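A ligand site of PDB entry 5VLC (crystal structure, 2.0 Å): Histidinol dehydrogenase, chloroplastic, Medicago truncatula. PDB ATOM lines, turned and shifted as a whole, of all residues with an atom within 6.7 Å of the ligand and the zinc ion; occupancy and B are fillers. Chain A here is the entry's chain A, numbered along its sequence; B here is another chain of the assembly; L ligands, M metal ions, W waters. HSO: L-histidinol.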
ATOM      1  N   VAL A 141      -2.187   4.624  20.973  1.00  0.00           N
ATOM      2  CA  VAL A 141      -1.225   4.471  19.914  1.00  0.00           C
ATOM      3  C   VAL A 141      -1.967   4.933  18.656  1.00  0.00           C
ATOM      4  O   VAL A 141      -2.856   4.224  18.149  1.00  0.00           O
ATOM      5  CB  VAL A 141      -0.780   2.993  19.815  1.00  0.00           C
ATOM      6  CG1 VAL A 141       0.158   2.786  18.636  1.00  0.00           C
ATOM      7  CG2 VAL A 141      -0.129   2.513  21.140  1.00  0.00           C
ATOM      8  N   LEU A 142      -1.623   6.112  18.134  1.00  0.00           N
ATOM      9  CA  LEU A 142      -2.301   6.673  16.941  1.00  0.00           C
ATOM     10  C   LEU A 142      -1.342   7.120  15.880  1.00  0.00           C
ATOM     11  O   LEU A 142      -1.365   8.277  15.451  1.00  0.00           O
ATOM     12  CB  LEU A 142      -3.206   7.813  17.332  1.00  0.00           C
ATOM     13  CG  LEU A 142      -4.439   7.330  18.074  1.00  0.00           C
ATOM     14  CD1 LEU A 142      -5.025   8.495  18.848  1.00  0.00           C
ATOM     15  CD2 LEU A 142      -5.456   6.766  17.082  1.00  0.00           C
ATOM     16  N   SER A 144      -1.532   6.436  12.883  1.00  0.00           N
ATOM     17  CA  SER A 144      -2.323   6.820  11.682  1.00  0.00           C
ATOM     18  C   SER A 144      -2.575   8.314  11.607  1.00  0.00           C
ATOM     19  O   SER A 144      -2.378   8.959  10.565  1.00  0.00           O
ATOM     20  CB  SER A 144      -3.651   6.012  11.582  1.00  0.00           C
ATOM     21  OG  SER A 144      -4.473   6.183  12.756  1.00  0.00           O
ATOM     22  N   THR A 145      -3.008   8.883  12.737  1.00  0.00           N
ATOM     23  CA  THR A 145      -3.255  10.307  12.843  1.00  0.00           C
ATOM     24  C   THR A 145      -1.988  11.099  12.647  1.00  0.00           C
ATOM     25  O   THR A 145      -2.015  12.163  12.035  1.00  0.00           O
ATOM     26  CB  THR A 145      -3.881  10.645  14.197  1.00  0.00           C
ATOM     27  OG1 THR A 145      -5.081   9.850  14.384  1.00  0.00           O
ATOM     28  CG2 THR A 145      -4.287  12.169  14.242  1.00  0.00           C
ATOM     29  N   SER A 245     -16.127  10.186  16.712  1.00  0.00           N
ATOM     30  CA  SER A 245     -16.218   9.633  15.369  1.00  0.00           C
ATOM     31  C   SER A 245     -17.663   9.153  15.051  1.00  0.00           C
ATOM     32  O   SER A 245     -18.468   8.844  15.954  1.00  0.00           O
ATOM     33  CB  SER A 245     -15.216   8.520  15.234  1.00  0.00           C
ATOM     34  OG  SER A 245     -13.974   8.993  15.709  1.00  0.00           O
ATOM     35  N   GLU A 246     -17.961   9.120  13.752  1.00  0.00           N
ATOM     36  CA  GLU A 246     -19.288   8.840  13.221  1.00  0.00           C
ATOM     37  C   GLU A 246     -19.190   8.047  11.966  1.00  0.00           C
ATOM     38  O   GLU A 246     -18.245   8.235  11.196  1.00  0.00           O
ATOM     39  CB  GLU A 246     -19.974  10.119  12.738  1.00  0.00           C
ATOM     40  CG  GLU A 246     -19.981  11.208  13.723  1.00  0.00           C
ATOM     41  CD  GLU A 246     -20.595  12.500  13.206  1.00  0.00           C
ATOM     42  OE1 GLU A 246     -20.701  12.767  11.960  1.00  0.00           O
ATOM     43  OE2 GLU A 246     -20.975  13.252  14.121  1.00  0.00           O
ATOM     44  N   SER A 266     -16.999  -1.099  13.312  1.00  0.00           N
ATOM     45  CA  SER A 266     -15.644  -0.544  13.143  1.00  0.00           C
ATOM     46  C   SER A 266     -15.476   0.843  13.815  1.00  0.00           C
ATOM     47  O   SER A 266     -14.514   1.076  14.524  1.00  0.00           O
ATOM     48  CB  SER A 266     -15.235  -0.526  11.654  1.00  0.00           C
ATOM     49  OG  SER A 266     -15.961   0.481  10.943  1.00  0.00           O
ATOM     50  N   GLN A 267     -16.415   1.755  13.597  1.00  0.00           N
ATOM     51  CA  GLN A 267     -16.364   3.077  14.290  1.00  0.00           C
ATOM     52  C   GLN A 267     -17.039   3.189  15.662  1.00  0.00           C
ATOM     53  O   GLN A 267     -16.673   4.057  16.470  1.00  0.00           O
ATOM     54  CB  GLN A 267     -16.818   4.181  13.341  1.00  0.00           C
ATOM     55  CG  GLN A 267     -16.090   4.102  11.986  1.00  0.00           C
ATOM     56  CD  GLN A 267     -14.550   3.916  12.024  1.00  0.00           C
ATOM     57  OE1 GLN A 267     -13.822   4.635  12.692  1.00  0.00           O
ATOM     58  NE2 GLN A 267     -14.061   2.921  11.276  1.00  0.00           N
ATOM     59  N   GLU A 269     -16.663   1.167  17.995  1.00  0.00           N
ATOM     60  CA  GLU A 269     -15.589   0.842  18.974  1.00  0.00           C
ATOM     61  C   GLU A 269     -14.694   2.009  19.357  1.00  0.00           C
ATOM     62  O   GLU A 269     -13.897   1.888  20.304  1.00  0.00           O
ATOM     63  CB  GLU A 269     -14.742  -0.372  18.549  1.00  0.00           C
ATOM     64  CG  GLU A 269     -13.721  -0.075  17.426  1.00  0.00           C
ATOM     65  CD  GLU A 269     -12.674  -1.152  17.217  1.00  0.00           C
ATOM     66  OE1 GLU A 269     -12.638  -2.149  18.004  1.00  0.00           O
ATOM     67  OE2 GLU A 269     -11.885  -1.005  16.250  1.00  0.00           O
ATOM     68  N   HIS A 270     -14.775   3.145  18.661  1.00  0.00           N
ATOM     69  CA  HIS A 270     -13.908   4.265  19.022  1.00  0.00           C
ATOM     70  C   HIS A 270     -14.174   4.733  20.455  1.00  0.00           C
ATOM     71  O   HIS A 270     -13.261   5.167  21.145  1.00  0.00           O
ATOM     72  CB  HIS A 270     -14.015   5.430  18.041  1.00  0.00           C
ATOM     73  CG  HIS A 270     -13.106   5.347  16.848  1.00  0.00           C
ATOM     74  ND1 HIS A 270     -11.747   5.456  16.958  1.00  0.00           N
ATOM     75  CD2 HIS A 270     -13.360   5.185  15.539  1.00  0.00           C
ATOM     76  CE1 HIS A 270     -11.194   5.367  15.769  1.00  0.00           C
ATOM     77  NE2 HIS A 270     -12.157   5.198  14.884  1.00  0.00           N
ATOM     78  N   GLU A 335     -19.601  12.386   9.357  1.00  0.00           N
ATOM     79  CA  GLU A 335     -18.168  12.391   9.190  1.00  0.00           C
ATOM     80  C   GLU A 335     -17.703  11.419   8.060  1.00  0.00           C
ATOM     81  O   GLU A 335     -16.879  11.772   7.183  1.00  0.00           O
ATOM     82  CB  GLU A 335     -17.498  11.996  10.498  1.00  0.00           C
ATOM     83  CG  GLU A 335     -15.978  12.248  10.494  1.00  0.00           C
ATOM     84  CD  GLU A 335     -15.235  11.493  11.595  1.00  0.00           C
ATOM     85  OE1 GLU A 335     -15.810  10.556  12.266  1.00  0.00           O
ATOM     86  OE2 GLU A 335     -14.020  11.874  11.788  1.00  0.00           O
ATOM     87  N   HIS A 336     -18.224  10.196   8.087  1.00  0.00           N
ATOM     88  CA  HIS A 336     -17.881   9.168   7.124  1.00  0.00           C
ATOM     89  C   HIS A 336     -19.174   8.593   6.609  1.00  0.00           C
ATOM     90  O   HIS A 336     -20.109   8.367   7.395  1.00  0.00           O
ATOM     91  CB  HIS A 336     -17.148   7.980   7.782  1.00  0.00           C
ATOM     92  CG  HIS A 336     -15.865   8.352   8.416  1.00  0.00           C
ATOM     93  ND1 HIS A 336     -15.767   8.637   9.760  1.00  0.00           N
ATOM     94  CD2 HIS A 336     -14.628   8.500   7.892  1.00  0.00           C
ATOM     95  CE1 HIS A 336     -14.498   8.945  10.038  1.00  0.00           C
ATOM     96  NE2 HIS A 336     -13.801   8.858   8.911  1.00  0.00           N
ATOM     97  N   GLU A 365     -14.672   1.533   5.825  1.00  0.00           N
ATOM     98  CA  GLU A 365     -14.073   2.757   6.267  1.00  0.00           C
ATOM     99  C   GLU A 365     -12.629   2.565   6.772  1.00  0.00           C
ATOM    100  O   GLU A 365     -11.819   3.476   6.641  1.00  0.00           O
ATOM    101  CB  GLU A 365     -14.918   3.379   7.378  1.00  0.00           C
ATOM    102  CG  GLU A 365     -14.195   4.604   7.963  1.00  0.00           C
ATOM    103  CD  GLU A 365     -14.934   5.349   9.049  1.00  0.00           C
ATOM    104  OE1 GLU A 365     -16.194   5.311   9.135  1.00  0.00           O
ATOM    105  OE2 GLU A 365     -14.211   6.003   9.832  1.00  0.00           O
ATOM    106  N   SER A 366     -12.332   1.386   7.348  1.00  0.00           N
ATOM    107  CA  SER A 366     -10.993   1.070   7.878  1.00  0.00           C
ATOM    108  C   SER A 366      -9.932   1.405   6.897  1.00  0.00           C
ATOM    109  O   SER A 366      -8.868   1.910   7.289  1.00  0.00           O
ATOM    110  CB  SER A 366     -10.871  -0.420   8.304  1.00  0.00           C
ATOM    111  OG  SER A 366     -11.909  -0.774   9.168  1.00  0.00           O
ATOM    112  N   GLY A 368      -9.754   3.910   4.693  1.00  0.00           N
ATOM    113  CA  GLY A 368      -9.533   5.359   4.774  1.00  0.00           C
ATOM    114  C   GLY A 368      -8.939   5.810   6.094  1.00  0.00           C
ATOM    115  O   GLY A 368      -8.077   6.701   6.109  1.00  0.00           O
ATOM    116  N   ASP A 369      -9.394   5.181   7.194  1.00  0.00           N
ATOM    117  CA  ASP A 369      -8.816   5.406   8.499  1.00  0.00           C
ATOM    118  C   ASP A 369      -7.295   5.223   8.499  1.00  0.00           C
ATOM    119  O   ASP A 369      -6.644   5.946   9.230  1.00  0.00           O
ATOM    120  CB  ASP A 369      -9.431   4.517   9.599  1.00  0.00           C
ATOM    121  CG  ASP A 369     -10.861   4.930  10.005  1.00  0.00           C
ATOM    122  OD1 ASP A 369     -11.409   5.946   9.459  1.00  0.00           O
ATOM    123  OD2 ASP A 369     -11.431   4.245  10.888  1.00  0.00           O
ATOM    124  N   TYR A 370      -6.833   4.237   7.750  1.00  0.00           N
ATOM    125  CA  TYR A 370      -5.463   3.846   7.733  1.00  0.00           C
ATOM    126  C   TYR A 370      -4.541   4.073   6.542  1.00  0.00           C
ATOM    127  O   TYR A 370      -3.507   4.612   6.722  1.00  0.00           O
ATOM    128  CB  TYR A 370      -5.378   2.378   8.148  1.00  0.00           C
ATOM    129  CG  TYR A 370      -5.751   2.153   9.574  1.00  0.00           C
ATOM    130  CD1 TYR A 370      -4.908   2.558  10.566  1.00  0.00           C
ATOM    131  CD2 TYR A 370      -6.945   1.600   9.917  1.00  0.00           C
ATOM    132  CE1 TYR A 370      -5.243   2.386  11.866  1.00  0.00           C
ATOM    133  CE2 TYR A 370      -7.284   1.442  11.220  1.00  0.00           C
ATOM    134  CZ  TYR A 370      -6.426   1.842  12.189  1.00  0.00           C
ATOM    135  OH  TYR A 370      -6.709   1.713  13.460  1.00  0.00           O
ATOM    136  N   ASN A 375      -7.621  11.511   3.915  1.00  0.00           N
ATOM    137  CA  ASN A 375      -7.346  11.964   5.251  1.00  0.00           C
ATOM    138  C   ASN A 375      -8.456  11.662   6.228  1.00  0.00           C
ATOM    139  O   ASN A 375      -9.583  11.969   5.948  1.00  0.00           O
ATOM    140  CB  ASN A 375      -7.111  13.463   5.227  1.00  0.00           C
ATOM    141  CG  ASN A 375      -6.210  13.913   6.354  1.00  0.00           C
ATOM    142  OD1 ASN A 375      -6.600  13.829   7.532  1.00  0.00           O
ATOM    143  ND2 ASN A 375      -5.012  14.378   6.000  1.00  0.00           N
ATOM    144  N   HIS A 376      -8.139  11.046   7.373  1.00  0.00           N
ATOM    145  CA  HIS A 376      -9.172  10.676   8.312  1.00  0.00           C
ATOM    146  C   HIS A 376      -9.509  11.760   9.334  1.00  0.00           C
ATOM    147  O   HIS A 376     -10.400  11.563  10.140  1.00  0.00           O
ATOM    148  CB  HIS A 376      -8.872   9.332   8.989  1.00  0.00           C
ATOM    149  CG  HIS A 376      -7.883   9.368  10.125  1.00  0.00           C
ATOM    150  ND1 HIS A 376      -6.971   8.360  10.308  1.00  0.00           N
ATOM    151  CD2 HIS A 376      -7.654  10.242  11.145  1.00  0.00           C
ATOM    152  CE1 HIS A 376      -6.242   8.599  11.372  1.00  0.00           C
ATOM    153  NE2 HIS A 376      -6.643   9.742  11.900  1.00  0.00           N
ATOM    154  N   VAL A 377      -8.803  12.885   9.324  1.00  0.00           N
ATOM    155  CA  VAL A 377      -9.069  14.006  10.203  1.00  0.00           C
ATOM    156  C   VAL A 377     -10.200  14.838   9.557  1.00  0.00           C
ATOM    157  O   VAL A 377      -9.977  15.640   8.644  1.00  0.00           O
ATOM    158  CB  VAL A 377      -7.823  14.849  10.506  1.00  0.00           C
ATOM    159  CG1 VAL A 377      -8.223  15.946  11.528  1.00  0.00           C
ATOM    160  CG2 VAL A 377      -6.740  13.951  11.121  1.00  0.00           C
ATOM    161  N   LEU A 378     -11.415  14.608  10.037  1.00  0.00           N
ATOM    162  CA  LEU A 378     -12.608  14.978   9.313  1.00  0.00           C
ATOM    163  C   LEU A 378     -13.639  15.675  10.207  1.00  0.00           C
ATOM    164  O   LEU A 378     -13.615  15.498  11.423  1.00  0.00           O
ATOM    165  CB  LEU A 378     -13.195  13.711   8.711  1.00  0.00           C
ATOM    166  CG  LEU A 378     -12.409  13.129   7.554  1.00  0.00           C
ATOM    167  CD1 LEU A 378     -12.803  11.665   7.439  1.00  0.00           C
ATOM    168  CD2 LEU A 378     -12.677  13.832   6.282  1.00  0.00           C
ATOM    169  N   GLU B 423      -2.865  -0.306  16.759  1.00  0.00           N
ATOM    170  CA  GLU B 423      -3.613   0.731  17.481  1.00  0.00           C
ATOM    171  C   GLU B 423      -4.604   0.146  18.489  1.00  0.00           C
ATOM    172  O   GLU B 423      -5.181   0.879  19.263  1.00  0.00           O
ATOM    173  CB  GLU B 423      -4.372   1.657  16.532  1.00  0.00           C
ATOM    174  CG  GLU B 423      -3.449   2.416  15.568  1.00  0.00           C
ATOM    175  CD  GLU B 423      -4.162   3.597  14.898  1.00  0.00           C
ATOM    176  OE1 GLU B 423      -5.461   3.576  14.863  1.00  0.00           O
ATOM    177  OE2 GLU B 423      -3.446   4.541  14.389  1.00  0.00           O
ATOM    178  N   LEU B 425      -7.406  -1.768  17.731  1.00  0.00           N
ATOM    179  CA  LEU B 425      -8.734  -1.470  17.162  1.00  0.00           C
ATOM    180  C   LEU B 425      -9.193  -2.632  16.316  1.00  0.00           C
ATOM    181  O   LEU B 425      -9.229  -2.590  15.092  1.00  0.00           O
ATOM    182  CB  LEU B 425      -8.708  -0.138  16.424  1.00  0.00           C
ATOM    183  CG  LEU B 425      -8.571   1.089  17.303  1.00  0.00           C
ATOM    184  CD1 LEU B 425      -8.582   2.360  16.491  1.00  0.00           C
ATOM    185  CD2 LEU B 425      -9.704   1.215  18.349  1.00  0.00           C
ATOM    186  N   HIS B 428     -12.002  -2.335  13.574  1.00  0.00           N
ATOM    187  CA  HIS B 428     -11.429  -1.810  12.316  1.00  0.00           C
ATOM    188  C   HIS B 428     -10.739  -2.882  11.516  1.00  0.00           C
ATOM    189  O   HIS B 428     -10.866  -2.968  10.317  1.00  0.00           O
ATOM    190  CB  HIS B 428     -10.398  -0.703  12.594  1.00  0.00           C
ATOM    191  CG  HIS B 428     -10.954   0.615  13.003  1.00  0.00           C
ATOM    192  ND1 HIS B 428     -11.537   0.853  14.222  1.00  0.00           N
ATOM    193  CD2 HIS B 428     -10.992   1.800  12.338  1.00  0.00           C
ATOM    194  CE1 HIS B 428     -11.922   2.106  14.293  1.00  0.00           C
ATOM    195  NE2 HIS B 428     -11.600   2.708  13.160  1.00  0.00           N
HETATM  196  N   HSO L   1     -12.096   6.774  12.384  1.00  0.00           N
HETATM  197  CA  HSO L   1     -11.203   7.866  12.927  1.00  0.00           C
HETATM  198  CB  HSO L   1      -9.790   7.639  12.509  1.00  0.00           C
HETATM  199  CG  HSO L   1      -9.155   6.380  12.971  1.00  0.00           C
HETATM  200  ND1 HSO L   1      -9.718   5.147  13.027  1.00  0.00           N
HETATM  201  CD2 HSO L   1      -7.879   6.142  13.453  1.00  0.00           C
HETATM  202  CE1 HSO L   1      -8.843   4.244  13.491  1.00  0.00           C
HETATM  203  NE2 HSO L   1      -7.692   4.843  13.770  1.00  0.00           N
HETATM  204  C   HSO L   1     -11.714   9.293  12.491  1.00  0.00           C
HETATM  205  O   HSO L   1     -11.563   9.425  11.088  1.00  0.00           O
HETATM  206 ZN    ZN M   1     -11.765   4.779  12.830  1.00  0.00          ZN
HETATM  207  O   HOH W   1     -13.118  11.434  14.492  1.00  0.00           O
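O of the ligand lies within hydrogen-bond range of O of His 376, 2.6 Å away. The side-chain carboxylate (OE1) of Glu 423 of chain B lies within hydrogen-bond range of a nitrogen (NE2) of the ligand (2.8 Å). An oxygen (O) of the ligand sits close to a ring nitrogen (NE2) of His 336, at 3.2 Å. A nitrogen (NE2) of the ligand is in hydrogen-bond range of the side-chain hydroxyl (OH) of Tyr 370, at 3.3 Å. OE2 of Glu 365 sits close to N of the ligand.
ND1 of His 376 is in hydrogen-bond range of O of Asp 369, at 2.7 Å. The side-chain amide nitrogen of Gln 267 lies close to the side-chain carboxylate of Glu 365, at 3.4 Å. The side-chain amide nitrogen of Gln 267 is in hydrogen-bond range of the side-chain hydroxyl of Ser 266, at 3.1 Å. The side-chain carboxylate (OE2) of Glu 269 is in hydrogen-bond range of a ring nitrogen (ND1) of His 428 of chain B, 2.8 Å away. OG1 of Thr 145 sits at hydrogen-bond distance from NE2 of His 376. The side-chain carboxylate (OE1) of Glu 423 of chain B sits at hydrogen-bond distance from the side-chain hydroxyl (OH) of Tyr 370, at 2.6 Å. O of Glu 246 is in hydrogen-bond range of ND1 of His 336 (2.9 Å). The backbone NH of Glu 335 lies within hydrogen-bond range of the side-chain carboxylate of Glu 246 (2.9 Å).
Merely in contact with the ligand: Ser 144, Ser 245, Glu 335 and Leu 425 of chain B. Hydrophobic or aromatic side chains within 4 Å of the ligand: His 270, His 336, Tyr 370, His 376, Leu 425 of chain B and His 428 of chain B. Of the 24 residues printed, 13 come within 4 Å of the ligand. Along chain A the residues within 4 Å of the ligand span positions 144 to 376.
Four residues have an atom within 4 Å of the zinc ion: Gln 267, His 270, Asp 369 and His 428 of chain B. Along chain A the residues within 4 Å of the zinc ion span positions 267 to 369. The nearest printed residue that does not touch the zinc ion is Glu 365 (4.1 Å).
The zinc ion is bound by the side-chain carboxylate (OD2) of Asp 369 (2.0 Å), the side-chain amide oxygen (OE1) of Gln 267 (2.1 Å), a nitrogen (N) of the ligand (2.1 Å), a nitrogen (ND1) of the ligand (2.1 Å), a ring nitrogen (NE2) of His 428 of chain B (2.1 Å) and a ring nitrogen (NE2) of His 270 (2.1 Å). The zinc ion has six donor atoms within binding distance.
Water W1 lies within hydrogen-bond range of OG of Ser 245 (2.9 Å) and OE2 of Glu 335 (2.9 Å).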
